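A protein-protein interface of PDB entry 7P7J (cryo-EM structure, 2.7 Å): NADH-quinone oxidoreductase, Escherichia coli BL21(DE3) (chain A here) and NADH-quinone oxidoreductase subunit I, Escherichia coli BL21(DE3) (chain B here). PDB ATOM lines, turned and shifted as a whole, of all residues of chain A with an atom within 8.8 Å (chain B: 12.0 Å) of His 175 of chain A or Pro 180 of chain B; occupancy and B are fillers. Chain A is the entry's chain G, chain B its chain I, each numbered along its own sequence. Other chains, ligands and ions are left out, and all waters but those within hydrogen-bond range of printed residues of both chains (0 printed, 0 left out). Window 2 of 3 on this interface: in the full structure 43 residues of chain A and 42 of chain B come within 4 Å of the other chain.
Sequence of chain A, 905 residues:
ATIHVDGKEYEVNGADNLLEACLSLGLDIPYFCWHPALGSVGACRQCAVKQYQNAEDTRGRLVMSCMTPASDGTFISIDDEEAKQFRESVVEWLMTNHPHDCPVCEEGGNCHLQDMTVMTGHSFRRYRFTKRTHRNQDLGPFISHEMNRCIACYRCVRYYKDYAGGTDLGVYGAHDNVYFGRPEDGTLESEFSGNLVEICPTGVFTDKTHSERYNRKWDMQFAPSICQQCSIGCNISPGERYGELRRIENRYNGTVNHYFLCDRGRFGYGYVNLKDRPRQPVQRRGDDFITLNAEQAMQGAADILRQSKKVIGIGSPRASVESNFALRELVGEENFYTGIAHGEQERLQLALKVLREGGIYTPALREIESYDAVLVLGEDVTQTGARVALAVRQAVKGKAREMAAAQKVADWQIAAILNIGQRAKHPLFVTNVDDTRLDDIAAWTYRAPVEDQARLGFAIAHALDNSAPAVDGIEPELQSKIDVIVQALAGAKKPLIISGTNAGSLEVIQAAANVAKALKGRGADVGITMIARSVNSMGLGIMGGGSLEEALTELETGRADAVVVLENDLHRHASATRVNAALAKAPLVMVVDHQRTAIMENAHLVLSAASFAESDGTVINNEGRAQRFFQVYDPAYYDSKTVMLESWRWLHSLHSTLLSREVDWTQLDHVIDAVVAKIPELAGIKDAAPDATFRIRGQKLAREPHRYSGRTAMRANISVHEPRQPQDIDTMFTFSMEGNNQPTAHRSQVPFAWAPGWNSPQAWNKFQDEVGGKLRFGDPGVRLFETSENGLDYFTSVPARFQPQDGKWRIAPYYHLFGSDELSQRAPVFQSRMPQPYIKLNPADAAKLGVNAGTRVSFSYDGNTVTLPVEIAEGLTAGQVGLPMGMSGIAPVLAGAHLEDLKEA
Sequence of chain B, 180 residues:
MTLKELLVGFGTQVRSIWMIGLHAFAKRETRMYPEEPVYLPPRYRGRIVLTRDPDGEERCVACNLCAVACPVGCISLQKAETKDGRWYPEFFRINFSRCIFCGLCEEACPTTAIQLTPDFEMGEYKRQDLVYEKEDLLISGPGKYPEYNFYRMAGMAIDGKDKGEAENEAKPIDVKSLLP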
ATOM      1  N   ASN A  97      -6.149  30.152  21.543  1.00  0.00           N
ATOM      2  CA  ASN A  97      -5.549  30.030  22.863  1.00  0.00           C
ATOM      3  C   ASN A  97      -5.733  31.283  23.701  1.00  0.00           C
ATOM      4  O   ASN A  97      -5.172  31.372  24.797  1.00  0.00           O
ATOM      5  CB  ASN A  97      -4.063  29.707  22.734  1.00  0.00           C
ATOM      6  CG  ASN A  97      -3.817  28.344  22.138  1.00  0.00           C
ATOM      7  OD1 ASN A  97      -4.320  27.339  22.630  1.00  0.00           O
ATOM      8  ND2 ASN A  97      -3.037  28.301  21.068  1.00  0.00           N
ATOM      9  N   ALA A 152       2.434  35.832  20.412  1.00  0.00           N
ATOM     10  CA  ALA A 152       3.757  35.508  19.875  1.00  0.00           C
ATOM     11  C   ALA A 152       4.071  36.330  18.626  1.00  0.00           C
ATOM     12  O   ALA A 152       4.412  35.799  17.571  1.00  0.00           O
ATOM     13  CB  ALA A 152       3.900  34.010  19.604  1.00  0.00           C
ATOM     14  N   TYR A 154       6.408  38.784  18.784  1.00  0.00           N
ATOM     15  CA  TYR A 154       7.835  39.070  18.944  1.00  0.00           C
ATOM     16  C   TYR A 154       8.161  40.560  18.930  1.00  0.00           C
ATOM     17  O   TYR A 154       9.313  40.933  18.718  1.00  0.00           O
ATOM     18  CB  TYR A 154       8.677  38.344  17.886  1.00  0.00           C
ATOM     19  CG  TYR A 154       8.689  36.845  18.044  1.00  0.00           C
ATOM     20  CD1 TYR A 154       7.690  36.062  17.485  1.00  0.00           C
ATOM     21  CD2 TYR A 154       9.697  36.210  18.750  1.00  0.00           C
ATOM     22  CE1 TYR A 154       7.691  34.695  17.630  1.00  0.00           C
ATOM     23  CE2 TYR A 154       9.708  34.842  18.896  1.00  0.00           C
ATOM     24  CZ  TYR A 154       8.701  34.091  18.333  1.00  0.00           C
ATOM     25  OH  TYR A 154       8.700  32.726  18.473  1.00  0.00           O
ATOM     26  N   TYR A 172      11.744  32.395  25.214  1.00  0.00           N
ATOM     27  CA  TYR A 172      12.130  31.063  25.635  1.00  0.00           C
ATOM     28  C   TYR A 172      11.112  30.060  25.125  1.00  0.00           C
ATOM     29  O   TYR A 172      10.040  30.416  24.635  1.00  0.00           O
ATOM     30  CB  TYR A 172      12.243  30.984  27.160  1.00  0.00           C
ATOM     31  CG  TYR A 172      12.757  32.263  27.744  1.00  0.00           C
ATOM     32  CD1 TYR A 172      14.082  32.634  27.578  1.00  0.00           C
ATOM     33  CD2 TYR A 172      11.913  33.126  28.418  1.00  0.00           C
ATOM     34  CE1 TYR A 172      14.556  33.810  28.091  1.00  0.00           C
ATOM     35  CE2 TYR A 172      12.378  34.304  28.934  1.00  0.00           C
ATOM     36  CZ  TYR A 172      13.701  34.642  28.767  1.00  0.00           C
ATOM     37  OH  TYR A 172      14.169  35.823  29.277  1.00  0.00           O
ATOM     38  N   GLY A 173      11.464  28.795  25.237  1.00  0.00           N
ATOM     39  CA  GLY A 173      10.544  27.758  24.855  1.00  0.00           C
ATOM     40  C   GLY A 173      10.567  27.472  23.368  1.00  0.00           C
ATOM     41  O   GLY A 173      11.529  27.747  22.649  1.00  0.00           O
ATOM     42  N   ALA A 174       9.449  26.928  22.905  1.00  0.00           N
ATOM     43  CA  ALA A 174       9.390  26.242  21.625  1.00  0.00           C
ATOM     44  C   ALA A 174       8.009  26.366  21.004  1.00  0.00           C
ATOM     45  O   ALA A 174       7.245  27.274  21.336  1.00  0.00           O
ATOM     46  CB  ALA A 174       9.777  24.772  21.785  1.00  0.00           C
ATOM     47  N   HIS A 175       7.681  25.395  20.158  1.00  0.00           N
ATOM     48  CA  HIS A 175       6.648  25.353  19.130  1.00  0.00           C
ATOM     49  C   HIS A 175       5.388  26.181  19.344  1.00  0.00           C
ATOM     50  O   HIS A 175       5.056  27.017  18.505  1.00  0.00           O
ATOM     51  CB  HIS A 175       6.237  23.892  19.000  1.00  0.00           C
ATOM     52  CG  HIS A 175       6.265  23.153  20.305  1.00  0.00           C
ATOM     53  ND1 HIS A 175       5.183  23.103  21.155  1.00  0.00           N
ATOM     54  CD2 HIS A 175       7.250  22.450  20.913  1.00  0.00           C
ATOM     55  CE1 HIS A 175       5.497  22.400  22.227  1.00  0.00           C
ATOM     56  NE2 HIS A 175       6.746  21.991  22.105  1.00  0.00           N
ATOM     57  N   ASP A 176       4.678  25.966  20.444  1.00  0.00           N
ATOM     58  CA  ASP A 176       3.537  26.802  20.789  1.00  0.00           C
ATOM     59  C   ASP A 176       3.568  27.172  22.260  1.00  0.00           C
ATOM     60  O   ASP A 176       2.590  27.725  22.776  1.00  0.00           O
ATOM     61  CB  ASP A 176       2.213  26.115  20.428  1.00  0.00           C
ATOM     62  CG  ASP A 176       1.952  24.870  21.248  1.00  0.00           C
ATOM     63  OD1 ASP A 176       2.921  24.179  21.622  1.00  0.00           O
ATOM     64  OD2 ASP A 176       0.767  24.578  21.509  1.00  0.00           O
ATOM     65  N   ASN A 177       4.669  26.874  22.943  1.00  0.00           N
ATOM     66  CA  ASN A 177       4.899  27.277  24.318  1.00  0.00           C
ATOM     67  C   ASN A 177       5.938  28.388  24.407  1.00  0.00           C
ATOM     68  O   ASN A 177       6.730  28.425  25.349  1.00  0.00           O
ATOM     69  CB  ASN A 177       5.332  26.075  25.152  1.00  0.00           C
ATOM     70  CG  ASN A 177       4.620  26.002  26.479  1.00  0.00           C
ATOM     71  OD1 ASN A 177       3.415  26.232  26.562  1.00  0.00           O
ATOM     72  ND2 ASN A 177       5.363  25.687  27.531  1.00  0.00           N
ATOM     73  N   VAL A 178       5.960  29.288  23.422  1.00  0.00           N
ATOM     74  CA  VAL A 178       6.897  30.404  23.450  1.00  0.00           C
ATOM     75  C   VAL A 178       6.547  31.342  24.595  1.00  0.00           C
ATOM     76  O   VAL A 178       5.395  31.767  24.751  1.00  0.00           O
ATOM     77  CB  VAL A 178       6.911  31.144  22.104  1.00  0.00           C
ATOM     78  CG1 VAL A 178       7.791  30.427  21.113  1.00  0.00           C
ATOM     79  CG2 VAL A 178       5.505  31.257  21.546  1.00  0.00           C
ATOM     80  N   TYR A 179       7.544  31.658  25.408  1.00  0.00           N
ATOM     81  CA  TYR A 179       7.401  32.521  26.567  1.00  0.00           C
ATOM     82  C   TYR A 179       8.206  33.787  26.336  1.00  0.00           C
ATOM     83  O   TYR A 179       9.308  33.736  25.794  1.00  0.00           O
ATOM     84  CB  TYR A 179       7.879  31.810  27.828  1.00  0.00           C
ATOM     85  CG  TYR A 179       7.291  32.331  29.111  1.00  0.00           C
ATOM     86  CD1 TYR A 179       7.855  33.417  29.760  1.00  0.00           C
ATOM     87  CD2 TYR A 179       6.182  31.729  29.680  1.00  0.00           C
ATOM     88  CE1 TYR A 179       7.328  33.893  30.936  1.00  0.00           C
ATOM     89  CE2 TYR A 179       5.649  32.197  30.860  1.00  0.00           C
ATOM     90  CZ  TYR A 179       6.223  33.281  31.481  1.00  0.00           C
ATOM     91  OH  TYR A 179       5.691  33.753  32.655  1.00  0.00           O
ATOM     92  N   ALA B 170      -5.905  24.205  29.561  1.00  0.00           N
ATOM     93  CA  ALA B 170      -4.917  23.209  29.929  1.00  0.00           C
ATOM     94  C   ALA B 170      -4.002  23.759  31.014  1.00  0.00           C
ATOM     95  O   ALA B 170      -3.891  24.970  31.209  1.00  0.00           O
ATOM     96  CB  ALA B 170      -4.097  22.785  28.712  1.00  0.00           C
ATOM     97  N   LYS B 171      -3.356  22.845  31.734  1.00  0.00           N
ATOM     98  CA  LYS B 171      -2.385  23.241  32.737  1.00  0.00           C
ATOM     99  C   LYS B 171      -1.194  23.924  32.067  1.00  0.00           C
ATOM    100  O   LYS B 171      -0.816  23.567  30.948  1.00  0.00           O
ATOM    101  CB  LYS B 171      -1.908  22.029  33.529  1.00  0.00           C
ATOM    102  CG  LYS B 171      -3.011  21.282  34.250  1.00  0.00           C
ATOM    103  CD  LYS B 171      -3.209  21.810  35.660  1.00  0.00           C
ATOM    104  CE  LYS B 171      -4.667  22.160  35.918  1.00  0.00           C
ATOM    105  NZ  LYS B 171      -4.969  22.256  37.371  1.00  0.00           N
ATOM    106  N   PRO B 172      -0.607  24.928  32.716  1.00  0.00           N
ATOM    107  CA  PRO B 172       0.531  25.629  32.110  1.00  0.00           C
ATOM    108  C   PRO B 172       1.759  24.734  32.036  1.00  0.00           C
ATOM    109  O   PRO B 172       2.164  24.124  33.027  1.00  0.00           O
ATOM    110  CB  PRO B 172       0.756  26.823  33.044  1.00  0.00           C
ATOM    111  CG  PRO B 172       0.106  26.444  34.320  1.00  0.00           C
ATOM    112  CD  PRO B 172      -1.048  25.571  33.965  1.00  0.00           C
ATOM    113  N   ILE B 173       2.345  24.662  30.847  1.00  0.00           N
ATOM    114  CA  ILE B 173       3.557  23.892  30.607  1.00  0.00           C
ATOM    115  C   ILE B 173       4.738  24.842  30.715  1.00  0.00           C
ATOM    116  O   ILE B 173       4.836  25.809  29.952  1.00  0.00           O
ATOM    117  CB  ILE B 173       3.525  23.209  29.232  1.00  0.00           C
ATOM    118  CG1 ILE B 173       2.302  22.303  29.116  1.00  0.00           C
ATOM    119  CG2 ILE B 173       4.800  22.423  29.003  1.00  0.00           C
ATOM    120  CD1 ILE B 173       2.090  21.755  27.728  1.00  0.00           C
ATOM    121  N   ASP B 174       5.627  24.576  31.664  1.00  0.00           N
ATOM    122  CA  ASP B 174       6.823  25.387  31.813  1.00  0.00           C
ATOM    123  C   ASP B 174       7.758  25.153  30.634  1.00  0.00           C
ATOM    124  O   ASP B 174       7.841  24.050  30.088  1.00  0.00           O
ATOM    125  CB  ASP B 174       7.529  25.056  33.128  1.00  0.00           C
ATOM    126  CG  ASP B 174       8.436  26.175  33.607  1.00  0.00           C
ATOM    127  OD1 ASP B 174       8.292  26.587  34.778  1.00  0.00           O
ATOM    128  OD2 ASP B 174       9.294  26.640  32.830  1.00  0.00           O
ATOM    129  N   VAL B 175       8.468  26.211  30.237  1.00  0.00           N
ATOM    130  CA  VAL B 175       9.401  26.099  29.122  1.00  0.00           C
ATOM    131  C   VAL B 175      10.628  25.285  29.497  1.00  0.00           C
ATOM    132  O   VAL B 175      11.352  24.817  28.613  1.00  0.00           O
ATOM    133  CB  VAL B 175       9.811  27.492  28.614  1.00  0.00           C
ATOM    134  CG1 VAL B 175       8.615  28.200  28.028  1.00  0.00           C
ATOM    135  CG2 VAL B 175      10.417  28.313  29.736  1.00  0.00           C
ATOM    136  N   LYS B 176      10.874  25.095  30.787  1.00  0.00           N
ATOM    137  CA  LYS B 176      11.998  24.311  31.269  1.00  0.00           C
ATOM    138  C   LYS B 176      11.694  22.821  31.323  1.00  0.00           C
ATOM    139  O   LYS B 176      12.578  22.040  31.687  1.00  0.00           O
ATOM    140  CB  LYS B 176      12.411  24.811  32.655  1.00  0.00           C
ATOM    141  CG  LYS B 176      13.302  26.049  32.624  1.00  0.00           C
ATOM    142  CD  LYS B 176      13.181  26.927  33.870  1.00  0.00           C
ATOM    143  CE  LYS B 176      12.743  26.164  35.111  1.00  0.00           C
ATOM    144  NZ  LYS B 176      13.851  25.352  35.684  1.00  0.00           N
ATOM    145  N   SER B 177      10.479  22.411  30.959  1.00  0.00           N
ATOM    146  CA  SER B 177      10.071  21.018  31.074  1.00  0.00           C
ATOM    147  C   SER B 177      10.816  20.137  30.079  1.00  0.00           C
ATOM    148  O   SER B 177      11.251  20.585  29.015  1.00  0.00           O
ATOM    149  CB  SER B 177       8.566  20.883  30.855  1.00  0.00           C
ATOM    150  OG  SER B 177       8.218  21.211  29.522  1.00  0.00           O
ATOM    151  N   LEU B 178      10.952  18.859  30.439  1.00  0.00           N
ATOM    152  CA  LEU B 178      11.772  17.931  29.671  1.00  0.00           C
ATOM    153  C   LEU B 178      11.111  17.492  28.372  1.00  0.00           C
ATOM    154  O   LEU B 178      11.810  17.098  27.433  1.00  0.00           O
ATOM    155  CB  LEU B 178      12.099  16.706  30.523  1.00  0.00           C
ATOM    156  CG  LEU B 178      12.693  17.012  31.896  1.00  0.00           C
ATOM    157  CD1 LEU B 178      12.777  15.749  32.728  1.00  0.00           C
ATOM    158  CD2 LEU B 178      14.059  17.649  31.742  1.00  0.00           C
ATOM    159  N   LEU B 179       9.785  17.533  28.305  1.00  0.00           N
ATOM    160  CA  LEU B 179       9.086  17.097  27.105  1.00  0.00           C
ATOM    161  C   LEU B 179       9.331  18.078  25.960  1.00  0.00           C
ATOM    162  O   LEU B 179       9.420  19.287  26.189  1.00  0.00           O
ATOM    163  CB  LEU B 179       7.589  16.973  27.376  1.00  0.00           C
ATOM    164  CG  LEU B 179       7.169  15.780  28.231  1.00  0.00           C
ATOM    165  CD1 LEU B 179       5.705  15.892  28.622  1.00  0.00           C
ATOM    166  CD2 LEU B 179       7.430  14.487  27.483  1.00  0.00           C
ATOM    167  N   PRO B 180       9.455  17.588  24.716  1.00  0.00           N
ATOM    168  CA  PRO B 180       9.663  18.449  23.546  1.00  0.00           C
ATOM    169  C   PRO B 180       8.473  19.358  23.256  1.00  0.00           C
ATOM    170  O   PRO B 180       7.350  19.005  23.614  1.00  0.00           O
ATOM    171  CB  PRO B 180       9.864  17.447  22.404  1.00  0.00           C
ATOM    172  CG  PRO B 180      10.270  16.182  23.067  1.00  0.00           C
ATOM    173  CD  PRO B 180       9.525  16.162  24.360  1.00  0.00           C
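The backbone carbonyl oxygen (O) of Tyr 179 of chain A sits at hydrogen-bond distance from the backbone NH (N) of Tyr 172 of chain A (2.8 Å).
ND1 of His 175 of chain A lies within hydrogen-bond range of OD1 of Asp 176 of chain A, 2.5 Å away.
OD2 of Asp 174 of chain B sits at hydrogen-bond distance from N of Lys 176 of chain B (3.0 Å).
OG of Ser 177 of chain B is in hydrogen-bond range of O of Asp 174 of chain B.
Pro 180 of chain B touches one residue of chain A.
Gly 173 of chain A touches just one residue of chain B: Val 175 (3.7 Å).
No residue of chain B comes within 4 Å of Asp 176 of chain A.
Of chain B, only Ile 173 (2.5 Å), Asp 174 (3.9 Å) and Val 175 (3.3 Å) come within 4 Å of Asn 177 of chain A.
No residue of chain B comes within 4 Å of Val 178 of chain A.
Of the printed residues of chain A, Val 175 of chain B touches Gly 173, Asn 177 and Tyr 179.
Printed residues of chain A within 4 Å of Asp 174 of chain B: Asn 177 (3.9 Å).
Of the printed residues of chain B, Tyr 179 of chain A touches Val 175.
Ala 152 of chain A touches none of the printed residues of chain B.
Lys 171 of chain B touches none of the printed residues of chain A.
The nearest residue of chain B that does not touch His 175 of chain A is Leu 179 of chain B (5.6 Å).
The nearest residue of chain A that does not touch Pro 180 of chain B is Ala 174 of chain A (5.8 Å).
Hydrophobic or aromatic side chains of chain B that line the printed part of chain A: Ile 173 and Val 175.
Printed residues of chain A that touch a printed residue of chain B: Gly 173, His 175, Asn 177 and Tyr 179.
Among the printed residues, 6 pairs touch across the chains.
Among the printed residues, no Asp or Glu carboxylate lies within 4 Å of a Lys or Arg side-chain nitrogen of the other chain.
The backbone carbonyl oxygen (O) of Pro 180 of chain B lies close to a ring nitrogen (NE2) of His 175 of chain A (3.4 Å).
ND2 of Asn 177 of chain A sits at hydrogen-bond distance from O of Ile 173 of chain B, at 2.5 Å.
Among the printed residues, merely in contact across the chains: Asn 177 of chain A with Val 175 of chain B, Tyr 179 of chain A with Val 175 of chain B, Gly 173 of chain A with Val 175 of chain B and Asn 177 of chain A with Asp 174 of chain B.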
